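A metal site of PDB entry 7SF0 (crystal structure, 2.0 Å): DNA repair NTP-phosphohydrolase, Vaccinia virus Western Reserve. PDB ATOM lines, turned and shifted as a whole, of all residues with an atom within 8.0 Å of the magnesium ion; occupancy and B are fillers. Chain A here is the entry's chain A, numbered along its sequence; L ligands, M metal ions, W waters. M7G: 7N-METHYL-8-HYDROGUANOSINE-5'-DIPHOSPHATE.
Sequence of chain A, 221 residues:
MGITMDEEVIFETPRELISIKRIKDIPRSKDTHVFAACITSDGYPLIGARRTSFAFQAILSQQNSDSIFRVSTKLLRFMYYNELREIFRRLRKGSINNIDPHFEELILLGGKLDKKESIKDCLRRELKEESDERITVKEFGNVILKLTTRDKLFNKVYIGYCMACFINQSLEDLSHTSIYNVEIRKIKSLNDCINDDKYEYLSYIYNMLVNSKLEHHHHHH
An oxygen (O2A) of the ligand sits close to a ring nitrogen (NE2) of His 33.
An oxygen (O2A) of the ligand is in salt-bridge range of the side-chain amino group (NZ) of Lys 112 (3.8 Å).
The side-chain amide oxygen of Asn 181 lies within hydrogen-bond range of the backbone NH of Glu 183, at 3.0 Å.
O of Glu 130 is in hydrogen-bond range of ND2 of Asn 181 (2.9 Å).
The side-chain carboxylate (OE1) of Glu 130 sits at hydrogen-bond distance from the backbone NH (N) of Gly 110 (3.2 Å).
OE2 of Glu 126 is in salt-bridge range of NH1 of Arg 125 (3.0 Å).
Water W3 bridges OE1 of Glu 129 (2.7 Å) and OE1 of Glu 183 (3.4 Å).
Merely in contact with the magnesium ion: Gly 110.
Within 4 Å of the magnesium ion: Gly 110, Glu 126, Glu 130 and Glu 183.
The nearest printed residue that does not touch the magnesium ion is Gly 111 (4.4 Å).
The magnesium ion is bound by water W1 (2.0 Å), water W2 (2.1 Å), water W3 (2.2 Å), OE2 of Glu 183 (2.2 Å), OE1 of Glu 126 (2.2 Å) and OE2 of Glu 130 (2.3 Å).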
ATOM      1  N   HIS A  33      16.263   2.775   8.162  1.00  0.00           N
ATOM      2  CA  HIS A  33      17.457   2.608   7.338  1.00  0.00           C
ATOM      3  C   HIS A  33      18.671   3.259   7.943  1.00  0.00           C
ATOM      4  O   HIS A  33      18.655   4.455   8.238  1.00  0.00           O
ATOM      5  CB  HIS A  33      17.335   3.257   5.948  1.00  0.00           C
ATOM      6  CG  HIS A  33      16.579   2.441   4.945  1.00  0.00           C
ATOM      7  ND1 HIS A  33      15.222   2.545   4.799  1.00  0.00           N
ATOM      8  CD2 HIS A  33      16.987   1.455   4.114  1.00  0.00           C
ATOM      9  CE1 HIS A  33      14.823   1.713   3.859  1.00  0.00           C
ATOM     10  NE2 HIS A  33      15.867   1.001   3.453  1.00  0.00           N
ATOM     11  N   VAL A  34      19.753   2.493   8.065  1.00  0.00           N
ATOM     12  CA  VAL A  34      21.033   3.076   8.429  1.00  0.00           C
ATOM     13  C   VAL A  34      22.012   2.958   7.250  1.00  0.00           C
ATOM     14  O   VAL A  34      22.281   1.865   6.747  1.00  0.00           O
ATOM     15  CB  VAL A  34      21.642   2.434   9.682  1.00  0.00           C
ATOM     16  CG1 VAL A  34      22.708   3.330  10.254  1.00  0.00           C
ATOM     17  CG2 VAL A  34      20.547   2.200  10.720  1.00  0.00           C
ATOM     18  N   ILE A 107      24.306   5.252  -4.500  1.00  0.00           N
ATOM     19  CA  ILE A 107      23.700   5.100  -3.183  1.00  0.00           C
ATOM     20  C   ILE A 107      24.756   4.870  -2.117  1.00  0.00           C
ATOM     21  O   ILE A 107      25.786   4.246  -2.366  1.00  0.00           O
ATOM     22  CB  ILE A 107      22.687   3.920  -3.133  1.00  0.00           C
ATOM     23  CG1 ILE A 107      23.361   2.606  -3.573  1.00  0.00           C
ATOM     24  CG2 ILE A 107      21.455   4.196  -3.989  1.00  0.00           C
ATOM     25  CD1 ILE A 107      22.511   1.392  -3.285  1.00  0.00           C
ATOM     26  N   LEU A 108      24.501   5.382  -0.917  1.00  0.00           N
ATOM     27  CA  LEU A 108      25.310   5.011   0.240  1.00  0.00           C
ATOM     28  C   LEU A 108      25.016   3.565   0.585  1.00  0.00           C
ATOM     29  O   LEU A 108      23.880   3.123   0.490  1.00  0.00           O
ATOM     30  CB  LEU A 108      25.007   5.918   1.427  1.00  0.00           C
ATOM     31  CG  LEU A 108      25.263   7.415   1.236  1.00  0.00           C
ATOM     32  CD1 LEU A 108      24.587   8.202   2.346  1.00  0.00           C
ATOM     33  CD2 LEU A 108      26.758   7.717   1.192  1.00  0.00           C
ATOM     34  N   LEU A 109      26.049   2.819   0.984  1.00  0.00           N
ATOM     35  CA  LEU A 109      25.836   1.444   1.407  1.00  0.00           C
ATOM     36  C   LEU A 109      25.045   1.448   2.711  1.00  0.00           C
ATOM     37  O   LEU A 109      25.013   2.467   3.384  1.00  0.00           O
ATOM     38  CB  LEU A 109      27.171   0.712   1.578  1.00  0.00           C
ATOM     39  CG  LEU A 109      28.114   0.793   0.376  1.00  0.00           C
ATOM     40  CD1 LEU A 109      29.436   0.081   0.641  1.00  0.00           C
ATOM     41  CD2 LEU A 109      27.427   0.220  -0.876  1.00  0.00           C
ATOM     42  N   GLY A 110      24.401   0.339   3.041  1.00  0.00           N
ATOM     43  CA  GLY A 110      23.632   0.275   4.275  1.00  0.00           C
ATOM     44  C   GLY A 110      22.255  -0.312   4.075  1.00  0.00           C
ATOM     45  O   GLY A 110      21.866  -0.615   2.942  1.00  0.00           O
ATOM     46  N   GLY A 111      21.496  -0.479   5.153  1.00  0.00           N
ATOM     47  CA  GLY A 111      20.203  -1.147   5.037  1.00  0.00           C
ATOM     48  C   GLY A 111      19.280  -1.075   6.253  1.00  0.00           C
ATOM     49  O   GLY A 111      19.475  -0.255   7.138  1.00  0.00           O
ATOM     50  N   LYS A 112      18.278  -1.962   6.255  1.00  0.00           N
ATOM     51  CA  LYS A 112      17.261  -2.075   7.318  1.00  0.00           C
ATOM     52  C   LYS A 112      17.864  -2.433   8.693  1.00  0.00           C
ATOM     53  O   LYS A 112      18.673  -3.342   8.823  1.00  0.00           O
ATOM     54  CB  LYS A 112      16.220  -3.151   6.929  1.00  0.00           C
ATOM     55  CG  LYS A 112      15.028  -2.722   6.039  1.00  0.00           C
ATOM     56  CD  LYS A 112      14.379  -1.434   6.522  1.00  0.00           C
ATOM     57  CE  LYS A 112      13.764  -0.695   5.363  1.00  0.00           C
ATOM     58  NZ  LYS A 112      13.074  -1.633   4.444  1.00  0.00           N
ATOM     59  N   CYS A 122      24.155  -3.540  12.780  1.00  0.00           N
ATOM     60  CA  CYS A 122      23.437  -3.385  11.525  1.00  0.00           C
ATOM     61  C   CYS A 122      24.371  -2.894  10.421  1.00  0.00           C
ATOM     62  O   CYS A 122      24.420  -3.482   9.341  1.00  0.00           O
ATOM     63  CB  CYS A 122      22.251  -2.428  11.684  1.00  0.00           C
ATOM     64  SG  CYS A 122      21.374  -2.052  10.141  1.00  0.00           S
ATOM     65  N   ARG A 125      26.891  -5.674   9.456  1.00  0.00           N
ATOM     66  CA  ARG A 125      26.251  -6.756   8.723  1.00  0.00           C
ATOM     67  C   ARG A 125      25.895  -6.342   7.301  1.00  0.00           C
ATOM     68  O   ARG A 125      26.169  -7.072   6.346  1.00  0.00           O
ATOM     69  CB  ARG A 125      24.998  -7.251   9.451  1.00  0.00           C
ATOM     70  CG  ARG A 125      24.228  -8.320   8.677  1.00  0.00           C
ATOM     71  CD  ARG A 125      22.932  -8.700   9.373  1.00  0.00           C
ATOM     72  NE  ARG A 125      22.123  -7.517   9.707  1.00  0.00           N
ATOM     73  CZ  ARG A 125      21.312  -6.903   8.853  1.00  0.00           C
ATOM     74  NH1 ARG A 125      21.197  -7.339   7.610  1.00  0.00           N
ATOM     75  NH2 ARG A 125      20.622  -5.831   9.247  1.00  0.00           N
ATOM     76  N   GLU A 126      25.273  -5.178   7.160  1.00  0.00           N
ATOM     77  CA  GLU A 126      24.847  -4.691   5.855  1.00  0.00           C
ATOM     78  C   GLU A 126      26.043  -4.403   4.957  1.00  0.00           C
ATOM     79  O   GLU A 126      26.021  -4.720   3.763  1.00  0.00           O
ATOM     80  CB  GLU A 126      23.966  -3.445   5.996  1.00  0.00           C
ATOM     81  CG  GLU A 126      22.566  -3.720   6.512  1.00  0.00           C
ATOM     82  CD  GLU A 126      21.671  -4.418   5.487  1.00  0.00           C
ATOM     83  OE1 GLU A 126      22.000  -4.360   4.284  1.00  0.00           O
ATOM     84  OE2 GLU A 126      20.643  -5.008   5.887  1.00  0.00           O
ATOM     85  N   LEU A 127      27.099  -3.817   5.525  1.00  0.00           N
ATOM     86  CA  LEU A 127      28.314  -3.562   4.756  1.00  0.00           C
ATOM     87  C   LEU A 127      28.909  -4.889   4.281  1.00  0.00           C
ATOM     88  O   LEU A 127      29.421  -4.984   3.169  1.00  0.00           O
ATOM     89  CB  LEU A 127      29.333  -2.771   5.563  1.00  0.00           C
ATOM     90  CG  LEU A 127      29.065  -1.269   5.737  1.00  0.00           C
ATOM     91  CD1 LEU A 127      30.068  -0.645   6.687  1.00  0.00           C
ATOM     92  CD2 LEU A 127      29.091  -0.570   4.397  1.00  0.00           C
ATOM     93  N   GLU A 129      27.157  -7.779   3.700  1.00  0.00           N
ATOM     94  CA  GLU A 129      26.287  -8.334   2.668  1.00  0.00           C
ATOM     95  C   GLU A 129      26.447  -7.628   1.327  1.00  0.00           C
ATOM     96  O   GLU A 129      26.440  -8.269   0.281  1.00  0.00           O
ATOM     97  CB  GLU A 129      24.823  -8.264   3.112  1.00  0.00           C
ATOM     98  CG  GLU A 129      24.533  -9.007   4.400  1.00  0.00           C
ATOM     99  CD  GLU A 129      23.095  -8.841   4.850  1.00  0.00           C
ATOM    100  OE1 GLU A 129      22.328  -8.144   4.141  1.00  0.00           O
ATOM    101  OE2 GLU A 129      22.731  -9.411   5.893  1.00  0.00           O
ATOM    102  N   GLU A 130      26.578  -6.308   1.358  1.00  0.00           N
ATOM    103  CA  GLU A 130      26.587  -5.526   0.128  1.00  0.00           C
ATOM    104  C   GLU A 130      27.959  -5.441  -0.542  1.00  0.00           C
ATOM    105  O   GLU A 130      28.070  -4.950  -1.663  1.00  0.00           O
ATOM    106  CB  GLU A 130      26.061  -4.125   0.402  1.00  0.00           C
ATOM    107  CG  GLU A 130      24.635  -4.146   0.926  1.00  0.00           C
ATOM    108  CD  GLU A 130      24.003  -2.777   0.989  1.00  0.00           C
ATOM    109  OE1 GLU A 130      24.706  -1.782   0.698  1.00  0.00           O
ATOM    110  OE2 GLU A 130      22.809  -2.693   1.336  1.00  0.00           O
ATOM    111  N   ASN A 181      26.604  -9.416  -5.519  1.00  0.00           N
ATOM    112  CA  ASN A 181      25.317  -9.545  -4.822  1.00  0.00           C
ATOM    113  C   ASN A 181      24.205  -8.795  -5.549  1.00  0.00           C
ATOM    114  O   ASN A 181      24.443  -8.055  -6.500  1.00  0.00           O
ATOM    115  CB  ASN A 181      25.438  -9.065  -3.379  1.00  0.00           C
ATOM    116  CG  ASN A 181      25.766  -7.596  -3.272  1.00  0.00           C
ATOM    117  OD1 ASN A 181      24.891  -6.746  -3.387  1.00  0.00           O
ATOM    118  ND2 ASN A 181      27.037  -7.297  -3.054  1.00  0.00           N
ATOM    119  N   GLU A 183      22.170  -6.433  -4.645  1.00  0.00           N
ATOM    120  CA  GLU A 183      21.846  -5.062  -4.266  1.00  0.00           C
ATOM    121  C   GLU A 183      22.763  -4.030  -4.913  1.00  0.00           C
ATOM    122  O   GLU A 183      22.341  -2.911  -5.203  1.00  0.00           O
ATOM    123  CB  GLU A 183      21.888  -4.913  -2.750  1.00  0.00           C
ATOM    124  CG  GLU A 183      20.766  -5.685  -2.039  1.00  0.00           C
ATOM    125  CD  GLU A 183      20.664  -5.358  -0.554  1.00  0.00           C
ATOM    126  OE1 GLU A 183      19.604  -5.632   0.029  1.00  0.00           O
ATOM    127  OE2 GLU A 183      21.644  -4.835   0.009  1.00  0.00           O
ATOM    128  N   ILE A 184      24.013  -4.411  -5.145  1.00  0.00           N
ATOM    129  CA  ILE A 184      25.054  -3.495  -5.609  1.00  0.00           C
ATOM    130  C   ILE A 184      25.783  -4.068  -6.832  1.00  0.00           C
ATOM    131  O   ILE A 184      26.206  -5.218  -6.822  1.00  0.00           O
ATOM    132  CB  ILE A 184      26.074  -3.215  -4.481  1.00  0.00           C
ATOM    133  CG1 ILE A 184      25.377  -2.575  -3.283  1.00  0.00           C
ATOM    134  CG2 ILE A 184      27.216  -2.353  -4.979  1.00  0.00           C
ATOM    135  CD1 ILE A 184      24.923  -1.173  -3.535  1.00  0.00           C
HETATM  136  PA  M7G L   1      14.061   1.049   0.331  1.00  0.00           P
HETATM  137  O1A M7G L   1      13.248   0.991  -0.959  1.00  0.00           O
HETATM  138  O2A M7G L   1      13.144   0.825   1.500  1.00  0.00           O
HETATM  139  O3A M7G L   1      15.203  -0.097   0.315  1.00  0.00           O
HETATM  140  O5' M7G L   1      14.758   2.465   0.475  1.00  0.00           O
HETATM  141  PB  M7G L   1      15.882  -0.678  -0.994  1.00  0.00           P
HETATM  142  O1B M7G L   1      16.617   0.429  -1.721  1.00  0.00           O
HETATM  143  O2B M7G L   1      16.853  -1.759  -0.617  1.00  0.00           O
HETATM  144  O3B M7G L   1      14.822  -1.251  -1.879  1.00  0.00           O
HETATM  145  C5' M7G L   1      16.175   2.521   0.684  1.00  0.00           C
HETATM  146  C4' M7G L   1      16.599   3.827   0.474  1.00  0.00           C
HETATM  147  O4' M7G L   1      16.881   4.001  -0.987  1.00  0.00           O
HETATM  148  C3' M7G L   1      15.421   4.870   0.785  1.00  0.00           C
HETATM  149  O3' M7G L   1      15.477   5.329   2.211  1.00  0.00           O
HETATM  150  C2' M7G L   1      15.647   5.806   0.006  1.00  0.00           C
HETATM  151  O2' M7G L   1      16.680   6.687   0.574  1.00  0.00           O
HETATM  152  C1' M7G L   1      16.264   5.115  -1.354  1.00  0.00           C
HETATM  153  N9  M7G L   1      15.286   4.827  -2.300  1.00  0.00           N
HETATM  154  C8  M7G L   1      14.573   3.577  -2.498  1.00  0.00           C
HETATM  155  N7  M7G L   1      13.659   3.776  -3.657  1.00  0.00           N
HETATM  156  CM7 M7G L   1      12.752   2.787  -4.195  1.00  0.00           C
HETATM  157  C5  M7G L   1      13.859   5.105  -4.092  1.00  0.00           C
HETATM  158  C6  M7G L   1      13.223   5.870  -5.227  1.00  0.00           C
HETATM  159  O6  M7G L   1      12.371   5.358  -5.939  1.00  0.00           O
HETATM  160  N1  M7G L   1      13.611   7.208  -5.454  1.00  0.00           N
HETATM  161  C2  M7G L   1      14.592   7.826  -4.624  1.00  0.00           C
HETATM  162  N2  M7G L   1      14.978   9.157  -4.858  1.00  0.00           N
HETATM  163  N3  M7G L   1      15.210   7.083  -3.544  1.00  0.00           N
HETATM  164  C4  M7G L   1      14.817   5.725  -3.298  1.00  0.00           C
HETATM  165 MG    MG M   1      21.357  -4.214   2.137  1.00  0.00          MG
HETATM  166  O   HOH W   1      20.108  -2.625   1.997  1.00  0.00           O
HETATM  167  O   HOH W   2      19.426  -5.076   2.370  1.00  0.00           O
HETATM  168  O   HOH W   3      22.211  -6.219   2.187  1.00  0.00           O
